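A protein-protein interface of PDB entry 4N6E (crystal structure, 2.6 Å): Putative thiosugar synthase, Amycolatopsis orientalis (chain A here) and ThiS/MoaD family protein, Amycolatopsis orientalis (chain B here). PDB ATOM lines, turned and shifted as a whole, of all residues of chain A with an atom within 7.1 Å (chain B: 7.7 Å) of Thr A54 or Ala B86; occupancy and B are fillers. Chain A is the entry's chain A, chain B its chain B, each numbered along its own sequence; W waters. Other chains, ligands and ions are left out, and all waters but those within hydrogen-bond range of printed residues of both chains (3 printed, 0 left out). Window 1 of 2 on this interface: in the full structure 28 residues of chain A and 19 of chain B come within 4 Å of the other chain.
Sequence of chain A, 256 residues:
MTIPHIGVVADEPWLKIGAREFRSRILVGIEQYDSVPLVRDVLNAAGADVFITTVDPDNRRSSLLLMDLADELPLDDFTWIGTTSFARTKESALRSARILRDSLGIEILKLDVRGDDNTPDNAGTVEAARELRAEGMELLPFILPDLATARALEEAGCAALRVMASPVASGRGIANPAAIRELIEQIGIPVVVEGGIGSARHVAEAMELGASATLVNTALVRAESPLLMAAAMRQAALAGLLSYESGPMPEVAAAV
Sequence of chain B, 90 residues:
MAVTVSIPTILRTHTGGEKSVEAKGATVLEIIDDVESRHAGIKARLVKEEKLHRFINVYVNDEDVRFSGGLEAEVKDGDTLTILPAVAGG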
ATOM      1  N   GLU A  31     -15.667 -27.561  18.338  1.00  0.00           N
ATOM      2  CA  GLU A  31     -15.215 -28.416  19.440  1.00  0.00           C
ATOM      3  C   GLU A  31     -16.281 -29.384  19.983  1.00  0.00           C
ATOM      4  O   GLU A  31     -15.949 -30.299  20.741  1.00  0.00           O
ATOM      5  CB  GLU A  31     -14.611 -27.575  20.571  1.00  0.00           C
ATOM      6  CG  GLU A  31     -15.532 -27.219  21.738  1.00  0.00           C
ATOM      7  CD  GLU A  31     -16.557 -26.166  21.410  1.00  0.00           C
ATOM      8  OE1 GLU A  31     -17.302 -25.756  22.333  1.00  0.00           O
ATOM      9  OE2 GLU A  31     -16.625 -25.746  20.242  1.00  0.00           O
ATOM     10  N   ILE A  52     -10.392 -23.725  13.384  1.00  0.00           N
ATOM     11  CA  ILE A  52     -10.099 -23.377  14.762  1.00  0.00           C
ATOM     12  C   ILE A  52      -9.552 -24.556  15.558  1.00  0.00           C
ATOM     13  O   ILE A  52     -10.205 -25.616  15.729  1.00  0.00           O
ATOM     14  CB  ILE A  52     -11.344 -22.832  15.479  1.00  0.00           C
ATOM     15  CG1 ILE A  52     -11.882 -21.601  14.730  1.00  0.00           C
ATOM     16  CG2 ILE A  52     -10.993 -22.473  16.921  1.00  0.00           C
ATOM     17  CD1 ILE A  52     -13.179 -21.046  15.267  1.00  0.00           C
ATOM     18  N   THR A  53      -8.371 -24.322  16.120  1.00  0.00           N
ATOM     19  CA  THR A  53      -7.569 -25.379  16.694  1.00  0.00           C
ATOM     20  C   THR A  53      -7.179 -25.033  18.129  1.00  0.00           C
ATOM     21  O   THR A  53      -7.048 -23.854  18.471  1.00  0.00           O
ATOM     22  CB  THR A  53      -6.354 -25.623  15.775  1.00  0.00           C
ATOM     23  OG1 THR A  53      -5.732 -26.866  16.110  1.00  0.00           O
ATOM     24  CG2 THR A  53      -5.345 -24.510  15.879  1.00  0.00           C
ATOM     25  N   THR A  54      -7.017 -26.044  18.980  1.00  0.00           N
ATOM     26  CA  THR A  54      -6.609 -25.797  20.368  1.00  0.00           C
ATOM     27  C   THR A  54      -5.974 -27.007  21.037  1.00  0.00           C
ATOM     28  O   THR A  54      -5.712 -28.024  20.405  1.00  0.00           O
ATOM     29  CB  THR A  54      -7.826 -25.314  21.212  1.00  0.00           C
ATOM     30  OG1 THR A  54      -7.396 -24.855  22.511  1.00  0.00           O
ATOM     31  CG2 THR A  54      -8.865 -26.421  21.376  1.00  0.00           C
ATOM     32  N   VAL A  55      -5.703 -26.877  22.330  1.00  0.00           N
ATOM     33  CA  VAL A  55      -5.312 -28.014  23.165  1.00  0.00           C
ATOM     34  C   VAL A  55      -6.148 -27.997  24.446  1.00  0.00           C
ATOM     35  O   VAL A  55      -6.658 -26.945  24.868  1.00  0.00           O
ATOM     36  CB  VAL A  55      -3.790 -28.028  23.475  1.00  0.00           C
ATOM     37  CG1 VAL A  55      -2.984 -28.290  22.204  1.00  0.00           C
ATOM     38  CG2 VAL A  55      -3.332 -26.721  24.104  1.00  0.00           C
ATOM     39  N   ASP A  56      -6.292 -29.174  25.047  1.00  0.00           N
ATOM     40  CA  ASP A  56      -7.194 -29.394  26.177  1.00  0.00           C
ATOM     41  C   ASP A  56      -6.414 -30.052  27.318  1.00  0.00           C
ATOM     42  O   ASP A  56      -6.572 -31.246  27.584  1.00  0.00           O
ATOM     43  CB  ASP A  56      -8.354 -30.291  25.711  1.00  0.00           C
ATOM     44  CG  ASP A  56      -9.609 -30.157  26.578  1.00  0.00           C
ATOM     45  OD1 ASP A  56      -9.524 -29.582  27.689  1.00  0.00           O
ATOM     46  OD2 ASP A  56     -10.690 -30.642  26.137  1.00  0.00           O
ATOM     47  N   PRO A  57      -5.537 -29.281  27.981  1.00  0.00           N
ATOM     48  CA  PRO A  57      -4.753 -29.859  29.076  1.00  0.00           C
ATOM     49  C   PRO A  57      -5.621 -30.556  30.143  1.00  0.00           C
ATOM     50  O   PRO A  57      -5.289 -31.672  30.563  1.00  0.00           O
ATOM     51  CB  PRO A  57      -4.033 -28.640  29.677  1.00  0.00           C
ATOM     52  CG  PRO A  57      -3.978 -27.640  28.578  1.00  0.00           C
ATOM     53  CD  PRO A  57      -5.215 -27.860  27.753  1.00  0.00           C
ATOM     54  N   SER A  63     -13.020 -33.302  22.041  1.00  0.00           N
ATOM     55  CA  SER A  63     -13.125 -32.744  20.699  1.00  0.00           C
ATOM     56  C   SER A  63     -12.166 -33.441  19.746  1.00  0.00           C
ATOM     57  O   SER A  63     -11.122 -33.925  20.153  1.00  0.00           O
ATOM     58  CB  SER A  63     -12.887 -31.226  20.713  1.00  0.00           C
ATOM     59  OG  SER A  63     -11.507 -30.897  20.770  1.00  0.00           O
ATOM     60  N   LEU A  64     -12.534 -33.484  18.474  1.00  0.00           N
ATOM     61  CA  LEU A  64     -11.850 -34.326  17.481  1.00  0.00           C
ATOM     62  C   LEU A  64     -10.352 -34.033  17.309  1.00  0.00           C
ATOM     63  O   LEU A  64      -9.916 -32.896  17.417  1.00  0.00           O
ATOM     64  CB  LEU A  64     -12.568 -34.201  16.134  1.00  0.00           C
ATOM     65  CG  LEU A  64     -14.007 -34.740  16.136  1.00  0.00           C
ATOM     66  CD1 LEU A  64     -14.813 -34.185  14.975  1.00  0.00           C
ATOM     67  CD2 LEU A  64     -14.020 -36.264  16.127  1.00  0.00           C
ATOM     68  N   LEU A  65      -9.573 -35.073  17.043  1.00  0.00           N
ATOM     69  CA  LEU A  65      -8.133 -34.943  16.805  1.00  0.00           C
ATOM     70  C   LEU A  65      -7.840 -34.375  15.426  1.00  0.00           C
ATOM     71  O   LEU A  65      -8.448 -34.807  14.448  1.00  0.00           O
ATOM     72  CB  LEU A  65      -7.476 -36.320  16.887  1.00  0.00           C
ATOM     73  CG  LEU A  65      -7.512 -36.995  18.252  1.00  0.00           C
ATOM     74  CD1 LEU A  65      -7.465 -38.513  18.141  1.00  0.00           C
ATOM     75  CD2 LEU A  65      -6.348 -36.469  19.071  1.00  0.00           C
ATOM     76  N   LEU A  66      -6.892 -33.443  15.338  1.00  0.00           N
ATOM     77  CA  LEU A  66      -6.423 -32.964  14.036  1.00  0.00           C
ATOM     78  C   LEU A  66      -5.898 -34.074  13.138  1.00  0.00           C
ATOM     79  O   LEU A  66      -5.999 -33.976  11.917  1.00  0.00           O
ATOM     80  CB  LEU A  66      -5.352 -31.879  14.180  1.00  0.00           C
ATOM     81  CG  LEU A  66      -5.927 -30.475  14.059  1.00  0.00           C
ATOM     82  CD1 LEU A  66      -6.948 -30.238  15.154  1.00  0.00           C
ATOM     83  CD2 LEU A  66      -4.830 -29.442  14.126  1.00  0.00           C
ATOM     84  N   MET A  67      -5.318 -35.111  13.734  1.00  0.00           N
ATOM     85  CA  MET A  67      -4.935 -36.313  12.984  1.00  0.00           C
ATOM     86  C   MET A  67      -6.084 -36.810  12.127  1.00  0.00           C
ATOM     87  O   MET A  67      -5.927 -37.004  10.925  1.00  0.00           O
ATOM     88  CB  MET A  67      -4.567 -37.436  13.938  1.00  0.00           C
ATOM     89  CG  MET A  67      -3.218 -37.283  14.587  1.00  0.00           C
ATOM     90  SD  MET A  67      -2.805 -38.828  15.405  1.00  0.00           S
ATOM     91  CE  MET A  67      -3.894 -38.768  16.817  1.00  0.00           C
ATOM     92  N   LEU A  69      -9.015 -35.287  11.487  1.00  0.00           N
ATOM     93  CA  LEU A  69      -9.598 -34.252  10.640  1.00  0.00           C
ATOM     94  C   LEU A  69      -8.753 -34.032   9.386  1.00  0.00           C
ATOM     95  O   LEU A  69      -9.284 -33.909   8.299  1.00  0.00           O
ATOM     96  CB  LEU A  69      -9.762 -32.944  11.428  1.00  0.00           C
ATOM     97  CG  LEU A  69     -10.847 -32.976  12.512  1.00  0.00           C
ATOM     98  CD1 LEU A  69     -10.600 -31.942  13.589  1.00  0.00           C
ATOM     99  CD2 LEU A  69     -12.210 -32.745  11.904  1.00  0.00           C
ATOM    100  N   TRP A  80      -5.641 -21.078   9.637  1.00  0.00           N
ATOM    101  CA  TRP A  80      -5.648 -21.753  10.936  1.00  0.00           C
ATOM    102  C   TRP A  80      -5.524 -20.728  12.034  1.00  0.00           C
ATOM    103  O   TRP A  80      -4.605 -19.918  12.017  1.00  0.00           O
ATOM    104  CB  TRP A  80      -4.462 -22.719  11.058  1.00  0.00           C
ATOM    105  CG  TRP A  80      -4.559 -23.955  10.222  1.00  0.00           C
ATOM    106  CD1 TRP A  80      -5.100 -24.068   8.978  1.00  0.00           C
ATOM    107  CD2 TRP A  80      -4.058 -25.242  10.559  1.00  0.00           C
ATOM    108  NE1 TRP A  80      -4.992 -25.359   8.531  1.00  0.00           N
ATOM    109  CE2 TRP A  80      -4.347 -26.099   9.484  1.00  0.00           C
ATOM    110  CE3 TRP A  80      -3.386 -25.757  11.669  1.00  0.00           C
ATOM    111  CZ2 TRP A  80      -3.986 -27.438   9.484  1.00  0.00           C
ATOM    112  CZ3 TRP A  80      -3.032 -27.082  11.671  1.00  0.00           C
ATOM    113  CH2 TRP A  80      -3.333 -27.912  10.587  1.00  0.00           C
ATOM    114  N   ILE A  81      -6.434 -20.746  12.990  1.00  0.00           N
ATOM    115  CA  ILE A  81      -6.274 -19.883  14.154  1.00  0.00           C
ATOM    116  C   ILE A  81      -6.374 -20.717  15.406  1.00  0.00           C
ATOM    117  O   ILE A  81      -7.001 -21.767  15.411  1.00  0.00           O
ATOM    118  CB  ILE A  81      -7.269 -18.706  14.182  1.00  0.00           C
ATOM    119  CG1 ILE A  81      -8.687 -19.174  14.498  1.00  0.00           C
ATOM    120  CG2 ILE A  81      -7.232 -17.952  12.857  1.00  0.00           C
ATOM    121  CD1 ILE A  81      -9.695 -18.040  14.560  1.00  0.00           C
ATOM    122  N   GLY A  82      -5.711 -20.256  16.457  1.00  0.00           N
ATOM    123  CA  GLY A  82      -5.682 -20.978  17.708  1.00  0.00           C
ATOM    124  C   GLY A  82      -6.770 -20.429  18.585  1.00  0.00           C
ATOM    125  O   GLY A  82      -7.178 -19.280  18.417  1.00  0.00           O
ATOM    126  N   THR A  83      -7.251 -21.230  19.525  1.00  0.00           N
ATOM    127  CA  THR A  83      -8.082 -20.654  20.573  1.00  0.00           C
ATOM    128  C   THR A  83      -7.651 -21.163  21.923  1.00  0.00           C
ATOM    129  O   THR A  83      -7.110 -22.258  22.010  1.00  0.00           O
ATOM    130  CB  THR A  83      -9.578 -20.945  20.367  1.00  0.00           C
ATOM    131  OG1 THR A  83     -10.311 -20.262  21.378  1.00  0.00           O
ATOM    132  CG2 THR A  83      -9.871 -22.424  20.484  1.00  0.00           C
ATOM    133  N   THR A  84      -7.917 -20.360  22.954  1.00  0.00           N
ATOM    134  CA  THR A  84      -7.615 -20.675  24.338  1.00  0.00           C
ATOM    135  C   THR A  84      -8.904 -20.819  25.137  1.00  0.00           C
ATOM    136  O   THR A  84      -8.894 -20.638  26.359  1.00  0.00           O
ATOM    137  CB  THR A  84      -6.752 -19.561  24.966  1.00  0.00           C
ATOM    138  OG1 THR A  84      -7.491 -18.326  25.051  1.00  0.00           O
ATOM    139  CG2 THR A  84      -5.508 -19.330  24.136  1.00  0.00           C
ATOM    140  N   SER A  85     -10.006 -21.153  24.460  1.00  0.00           N
ATOM    141  CA  SER A  85     -11.333 -21.201  25.099  1.00  0.00           C
ATOM    142  C   SER A  85     -11.580 -22.368  26.067  1.00  0.00           C
ATOM    143  O   SER A  85     -12.535 -22.312  26.834  1.00  0.00           O
ATOM    144  CB  SER A  85     -12.469 -21.163  24.048  1.00  0.00           C
ATOM    145  OG  SER A  85     -12.403 -22.238  23.103  1.00  0.00           O
ATOM    146  N   PHE A  86     -10.752 -23.417  26.062  1.00  0.00           N
ATOM    147  CA  PHE A  86     -10.872 -24.445  27.118  1.00  0.00           C
ATOM    148  C   PHE A  86     -10.210 -23.998  28.423  1.00  0.00           C
ATOM    149  O   PHE A  86     -10.494 -24.571  29.480  1.00  0.00           O
ATOM    150  CB  PHE A  86     -10.271 -25.805  26.723  1.00  0.00           C
ATOM    151  CG  PHE A  86     -11.014 -26.538  25.634  1.00  0.00           C
ATOM    152  CD1 PHE A  86     -12.405 -26.578  25.595  1.00  0.00           C
ATOM    153  CD2 PHE A  86     -10.304 -27.235  24.656  1.00  0.00           C
ATOM    154  CE1 PHE A  86     -13.067 -27.275  24.586  1.00  0.00           C
ATOM    155  CE2 PHE A  86     -10.966 -27.930  23.641  1.00  0.00           C
ATOM    156  CZ  PHE A  86     -12.344 -27.946  23.607  1.00  0.00           C
ATOM    157  N   ALA A  87      -9.321 -23.009  28.375  1.00  0.00           N
ATOM    158  CA  ALA A  87      -8.589 -22.614  29.591  1.00  0.00           C
ATOM    159  C   ALA A  87      -9.537 -21.959  30.591  1.00  0.00           C
ATOM    160  O   ALA A  87     -10.503 -21.347  30.182  1.00  0.00           O
ATOM    161  CB  ALA A  87      -7.438 -21.674  29.248  1.00  0.00           C
ATOM    162  N   SER A  96      -1.508 -22.221  26.828  1.00  0.00           N
ATOM    163  CA  SER A  96      -2.100 -22.795  25.606  1.00  0.00           C
ATOM    164  C   SER A  96      -1.773 -21.973  24.326  1.00  0.00           C
ATOM    165  O   SER A  96      -1.445 -22.544  23.268  1.00  0.00           O
ATOM    166  CB  SER A  96      -3.621 -22.955  25.766  1.00  0.00           C
ATOM    167  OG  SER A  96      -3.957 -24.169  26.444  1.00  0.00           O
ATOM    168  N   LEU A 100       0.345 -23.512  21.183  1.00  0.00           N
ATOM    169  CA  LEU A 100      -0.156 -23.503  19.807  1.00  0.00           C
ATOM    170  C   LEU A 100       0.833 -22.863  18.857  1.00  0.00           C
ATOM    171  O   LEU A 100       0.959 -23.284  17.707  1.00  0.00           O
ATOM    172  CB  LEU A 100      -1.518 -22.812  19.719  1.00  0.00           C
ATOM    173  CG  LEU A 100      -2.628 -23.583  20.434  1.00  0.00           C
ATOM    174  CD1 LEU A 100      -3.841 -22.705  20.682  1.00  0.00           C
ATOM    175  CD2 LEU A 100      -3.012 -24.823  19.637  1.00  0.00           C
ATOM    176  N   SER A 103       3.963 -25.553  18.639  1.00  0.00           N
ATOM    177  CA  SER A 103       3.624 -26.853  18.072  1.00  0.00           C
ATOM    178  C   SER A 103       3.094 -26.817  16.622  1.00  0.00           C
ATOM    179  O   SER A 103       3.336 -27.746  15.849  1.00  0.00           O
ATOM    180  CB  SER A 103       2.583 -27.528  18.967  1.00  0.00           C
ATOM    181  OG  SER A 103       1.373 -26.779  18.989  1.00  0.00           O
ATOM    182  N   LEU A 104       2.347 -25.772  16.271  1.00  0.00           N
ATOM    183  CA  LEU A 104       1.708 -25.667  14.946  1.00  0.00           C
ATOM    184  C   LEU A 104       2.097 -24.419  14.185  1.00  0.00           C
ATOM    185  O   LEU A 104       1.694 -24.261  13.038  1.00  0.00           O
ATOM    186  CB  LEU A 104       0.173 -25.702  15.067  1.00  0.00           C
ATOM    187  CG  LEU A 104      -0.438 -26.896  15.805  1.00  0.00           C
ATOM    188  CD1 LEU A 104      -1.956 -26.799  15.886  1.00  0.00           C
ATOM    189  CD2 LEU A 104      -0.025 -28.181  15.122  1.00  0.00           C
ATOM    190  N   ILE B  10      -9.498 -38.736  25.013  1.00  0.00           N
ATOM    191  CA  ILE B  10      -9.794 -39.185  23.657  1.00  0.00           C
ATOM    192  C   ILE B  10      -9.019 -40.464  23.291  1.00  0.00           C
ATOM    193  O   ILE B  10      -9.434 -41.199  22.398  1.00  0.00           O
ATOM    194  CB  ILE B  10      -9.527 -38.067  22.610  1.00  0.00           C
ATOM    195  CG1 ILE B  10      -9.915 -36.665  23.152  1.00  0.00           C
ATOM    196  CG2 ILE B  10     -10.300 -38.356  21.318  1.00  0.00           C
ATOM    197  CD1 ILE B  10      -8.816 -35.860  23.836  1.00  0.00           C
ATOM    198  N   ARG B  54       3.179 -34.885  14.060  1.00  0.00           N
ATOM    199  CA  ARG B  54       3.108 -33.413  14.032  1.00  0.00           C
ATOM    200  C   ARG B  54       1.944 -32.824  14.875  1.00  0.00           C
ATOM    201  O   ARG B  54       2.052 -31.714  15.381  1.00  0.00           O
ATOM    202  CB  ARG B  54       3.018 -32.920  12.583  1.00  0.00           C
ATOM    203  CG  ARG B  54       1.747 -33.357  11.849  1.00  0.00           C
ATOM    204  CD  ARG B  54       1.611 -32.747  10.450  1.00  0.00           C
ATOM    205  NE  ARG B  54       1.796 -31.289  10.434  1.00  0.00           N
ATOM    206  CZ  ARG B  54       1.492 -30.492   9.408  1.00  0.00           C
ATOM    207  NH1 ARG B  54       0.952 -30.981   8.294  1.00  0.00           N
ATOM    208  NH2 ARG B  54       1.715 -29.186   9.510  1.00  0.00           N
ATOM    209  N   PHE B  55       0.852 -33.578  15.025  1.00  0.00           N
ATOM    210  CA  PHE B  55      -0.331 -33.143  15.764  1.00  0.00           C
ATOM    211  C   PHE B  55      -0.435 -33.751  17.147  1.00  0.00           C
ATOM    212  O   PHE B  55      -1.532 -33.821  17.723  1.00  0.00           O
ATOM    213  CB  PHE B  55      -1.590 -33.470  14.963  1.00  0.00           C
ATOM    214  CG  PHE B  55      -1.684 -32.716  13.671  1.00  0.00           C
ATOM    215  CD1 PHE B  55      -1.298 -31.385  13.609  1.00  0.00           C
ATOM    216  CD2 PHE B  55      -2.143 -33.329  12.520  1.00  0.00           C
ATOM    217  CE1 PHE B  55      -1.364 -30.679  12.422  1.00  0.00           C
ATOM    218  CE2 PHE B  55      -2.211 -32.628  11.325  1.00  0.00           C
ATOM    219  CZ  PHE B  55      -1.823 -31.297  11.275  1.00  0.00           C
ATOM    220  N   ILE B  56       0.713 -34.156  17.686  1.00  0.00           N
ATOM    221  CA  ILE B  56       0.796 -34.665  19.040  1.00  0.00           C
ATOM    222  C   ILE B  56       1.869 -33.895  19.775  1.00  0.00           C
ATOM    223  O   ILE B  56       2.902 -33.607  19.208  1.00  0.00           O
ATOM    224  CB  ILE B  56       1.136 -36.177  19.033  1.00  0.00           C
ATOM    225  CG1 ILE B  56      -0.079 -36.975  18.563  1.00  0.00           C
ATOM    226  CG2 ILE B  56       1.562 -36.666  20.413  1.00  0.00           C
ATOM    227  CD1 ILE B  56      -1.223 -36.979  19.550  1.00  0.00           C
ATOM    228  N   ASN B  57       1.619 -33.559  21.032  1.00  0.00           N
ATOM    229  CA  ASN B  57       2.634 -32.949  21.880  1.00  0.00           C
ATOM    230  C   ASN B  57       2.883 -33.817  23.083  1.00  0.00           C
ATOM    231  O   ASN B  57       1.942 -34.359  23.665  1.00  0.00           O
ATOM    232  CB  ASN B  57       2.191 -31.575  22.359  1.00  0.00           C
ATOM    233  CG  ASN B  57       1.658 -30.725  21.238  1.00  0.00           C
ATOM    234  OD1 ASN B  57       2.412 -30.307  20.362  1.00  0.00           O
ATOM    235  ND2 ASN B  57       0.348 -30.482  21.242  1.00  0.00           N
ATOM    236  N   ILE B  83       0.650 -36.530  27.442  1.00  0.00           N
ATOM    237  CA  ILE B  83       0.314 -36.527  26.018  1.00  0.00           C
ATOM    238  C   ILE B  83      -0.818 -35.538  25.758  1.00  0.00           C
ATOM    239  O   ILE B  83      -1.880 -35.625  26.361  1.00  0.00           O
ATOM    240  CB  ILE B  83      -0.127 -37.911  25.539  1.00  0.00           C
ATOM    241  CG1 ILE B  83       0.895 -38.966  25.967  1.00  0.00           C
ATOM    242  CG2 ILE B  83      -0.305 -37.901  24.025  1.00  0.00           C
ATOM    243  CD1 ILE B  83       0.566 -40.381  25.525  1.00  0.00           C
ATOM    244  N   LEU B  84      -0.580 -34.605  24.849  1.00  0.00           N
ATOM    245  CA  LEU B  84      -1.483 -33.476  24.631  1.00  0.00           C
ATOM    246  C   LEU B  84      -1.681 -33.256  23.129  1.00  0.00           C
ATOM    247  O   LEU B  84      -0.904 -32.541  22.492  1.00  0.00           O
ATOM    248  CB  LEU B  84      -0.887 -32.242  25.287  1.00  0.00           C
ATOM    249  CG  LEU B  84      -1.748 -30.998  25.392  1.00  0.00           C
ATOM    250  CD1 LEU B  84      -2.826 -31.165  26.457  1.00  0.00           C
ATOM    251  CD2 LEU B  84      -0.864 -29.801  25.710  1.00  0.00           C
ATOM    252  N   PRO B  85      -2.720 -33.886  22.554  1.00  0.00           N
ATOM    253  CA  PRO B  85      -2.941 -33.779  21.120  1.00  0.00           C
ATOM    254  C   PRO B  85      -3.595 -32.458  20.694  1.00  0.00           C
ATOM    255  O   PRO B  85      -4.335 -31.841  21.458  1.00  0.00           O
ATOM    256  CB  PRO B  85      -3.863 -34.956  20.821  1.00  0.00           C
ATOM    257  CG  PRO B  85      -4.601 -35.193  22.071  1.00  0.00           C
ATOM    258  CD  PRO B  85      -3.727 -34.746  23.204  1.00  0.00           C
ATOM    259  N   ALA B  86      -3.281 -32.045  19.474  1.00  0.00           N
ATOM    260  CA  ALA B  86      -3.935 -30.926  18.823  1.00  0.00           C
ATOM    261  C   ALA B  86      -5.378 -31.310  18.572  1.00  0.00           C
ATOM    262  O   ALA B  86      -5.640 -32.386  18.059  1.00  0.00           O
ATOM    263  CB  ALA B  86      -3.245 -30.622  17.502  1.00  0.00           C
ATOM    264  N   VAL B  87      -6.314 -30.437  18.938  1.00  0.00           N
ATOM    265  CA  VAL B  87      -7.727 -30.744  18.770  1.00  0.00           C
ATOM    266  C   VAL B  87      -8.560 -29.608  18.175  1.00  0.00           C
ATOM    267  O   VAL B  87      -8.135 -28.453  18.111  1.00  0.00           O
ATOM    268  CB  VAL B  87      -8.360 -31.198  20.091  1.00  0.00           C
ATOM    269  CG1 VAL B  87      -7.643 -32.426  20.629  1.00  0.00           C
ATOM    270  CG2 VAL B  87      -8.361 -30.081  21.115  1.00  0.00           C
ATOM    271  N   ALA B  88      -9.749 -29.988  17.716  1.00  0.00           N
ATOM    272  CA  ALA B  88     -10.735 -29.061  17.210  1.00  0.00           C
ATOM    273  C   ALA B  88     -11.089 -28.066  18.300  1.00  0.00           C
ATOM    274  O   ALA B  88     -11.376 -28.455  19.428  1.00  0.00           O
ATOM    275  CB  ALA B  88     -11.986 -29.818  16.777  1.00  0.00           C
ATOM    276  N   GLY B  89     -11.076 -26.783  17.945  1.00  0.00           N
ATOM    277  CA  GLY B  89     -11.359 -25.723  18.902  1.00  0.00           C
ATOM    278  C   GLY B  89     -12.714 -25.098  18.689  1.00  0.00           C
ATOM    279  O   GLY B  89     -13.274 -25.171  17.594  1.00  0.00           O
ATOM    280  N   GLY B  90     -13.232 -24.489  19.756  1.00  0.00           N
ATOM    281  CA  GLY B  90     -14.521 -23.786  19.736  1.00  0.00           C
ATOM    282  C   GLY B  90     -14.394 -22.273  19.845  1.00  0.00           C
ATOM    283  O   GLY B  90     -15.368 -21.529  19.655  1.00  0.00           O
ATOM    284  OXT GLY B  90     -13.316 -21.752  20.142  1.00  0.00           O
HETATM  285  O   HOH W   1      -4.181 -34.920  16.857  1.00  0.00           O
HETATM  286  O   HOH W   2      -5.470 -31.285  24.147  1.00  0.00           O
HETATM  287  O   HOH W   3     -12.091 -24.893  23.003  1.00  0.00           O
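The backbone NH of Glu A31 lies within hydrogen-bond range of the backbone carbonyl oxygen of Gly B89, 3.5 Å away. The backbone carbonyl oxygen (O) of Ile A52 lies within hydrogen-bond range of the backbone NH (N) of Gly B89, 2.7 Å away. The backbone carbonyl oxygen of Val B87 lies within hydrogen-bond range of the backbone NH of Thr A54. The side-chain hydroxyl (OG) of Ser A63 lies within hydrogen-bond range of the backbone carbonyl oxygen (O) of Ala B88, at 2.8 Å. N of Ala B88 sits at hydrogen-bond distance from O of Leu A64, 2.9 Å away. The backbone NH (N) of Leu A66 is in hydrogen-bond range of the backbone carbonyl oxygen (O) of Ala B86, at 3.2 Å. OG of Ser A85 lies within hydrogen-bond range of OXT of Gly B90 (3.1 Å).
The backbone NH of Thr A53 is in hydrogen-bond range of the backbone carbonyl oxygen of Ile A81 (3.0 Å). The backbone carbonyl oxygen (O) of Thr A53 sits at hydrogen-bond distance from the backbone NH (N) of Thr A83 (2.8 Å). OG1 of Thr A54 sits at hydrogen-bond distance from O of Thr A83 (2.7 Å). The side-chain hydroxyl of Thr A83 is in hydrogen-bond range of the backbone NH of Ser A85 (3.2 Å). The backbone carbonyl oxygen (O) of Phe B55 sits at hydrogen-bond distance from the backbone NH (N) of Ala B86, at 3.0 Å. The backbone carbonyl oxygen (O) of Leu B84 sits at hydrogen-bond distance from the side-chain amide nitrogen (ND2) of Asn B57 (2.7 Å).
Among the printed residues, merely in contact across the chains: Glu A31 with Ala B88 (3.5 Å), Glu A31 with Gly B90 (2.9 Å), Ile A52 with Ala B88 (3.7 Å), Thr A53 with Val B87 (3.4 Å), Thr A53 with Gly B89 (3.98 Å), Thr A54 with Ala B86 (3.8 Å), Thr A54 with Ala B88 (3.8 Å), Thr A54 with Gly B89 (3.6 Å), Val A55 with Pro B85 (3.9 Å), Asp A56 with Leu B84 (3.9 Å), Pro A57 with Leu B84 (3.5 Å), Ser A63 with Val B87 (3.2 Å), Leu A64 with Val B87 (3.4 Å), Leu A65 with Pro B85 (3.4 Å), Leu A65 with Ala B86 (3.8 Å), Leu A66 with Phe B55 (3.8 Å), Leu A66 with Val B87 (3.5 Å), Leu A66 with Ala B88 (3.8 Å), Met A67 with Phe B55 (3.8 Å), Trp A80 with Phe B55 (3.8 Å), Thr A83 with Gly B89 (3.9 Å), Thr A83 with Gly B90 (3.5 Å), Ser A103 with Asn B57 (3.1 Å) and Leu A104 with Phe B55 (3.8 Å).
Thr A54 touches four residues of chain B. Ala B86 touches just these residues of chain A: Thr A54, Leu A65 and Leu A66. Of the printed residues of chain B, Glu A31 touches Ala B88 (3.5 Å), Gly B89 (3.5 Å) and Gly B90 (2.9 Å). Of the printed residues of chain A, Gly B90 touches Glu A31, Thr A83 and Ser A85. The nearest residue of chain B that does not touch Thr A54 is Pro B85 (4.2 Å). The nearest printed residue of chain A that does not touch Ala B86 is Leu A104 (4.3 Å). The nearest printed residue of chain B that does not touch Ile A52 is Gly B90 (4.04 Å).
Of the 25 printed residues of chain A, 17 touch a printed residue of chain B. Hydrophobic or aromatic side chains of chain A within 4 Å of the printed part of chain B: Ile A52, Val A55, Leu A65, Leu A66, Trp A80 and Leu A104. Hydrophobic or aromatic side chains of chain B that line the printed part of chain A: Phe B55, Leu B84, Pro B85, Ala B86, Val B87 and Ala B88. Among the printed residues, no Asp or Glu carboxylate lies within 4 Å of a Lys or Arg side-chain nitrogen of the other chain.
Water W2 bridges N of Asp A56 (2.4 Å) and O of Pro B85 (3.0 Å). Water W3 lies within hydrogen-bond range of OG of Ser A85 and N of Gly B90. Water W1 lies within hydrogen-bond range of O of Phe B55 (3.0 Å), O of Ala B86 (3.2 Å), N of Met A67 (3.3 Å) and N of Leu A66 (3.4 Å).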
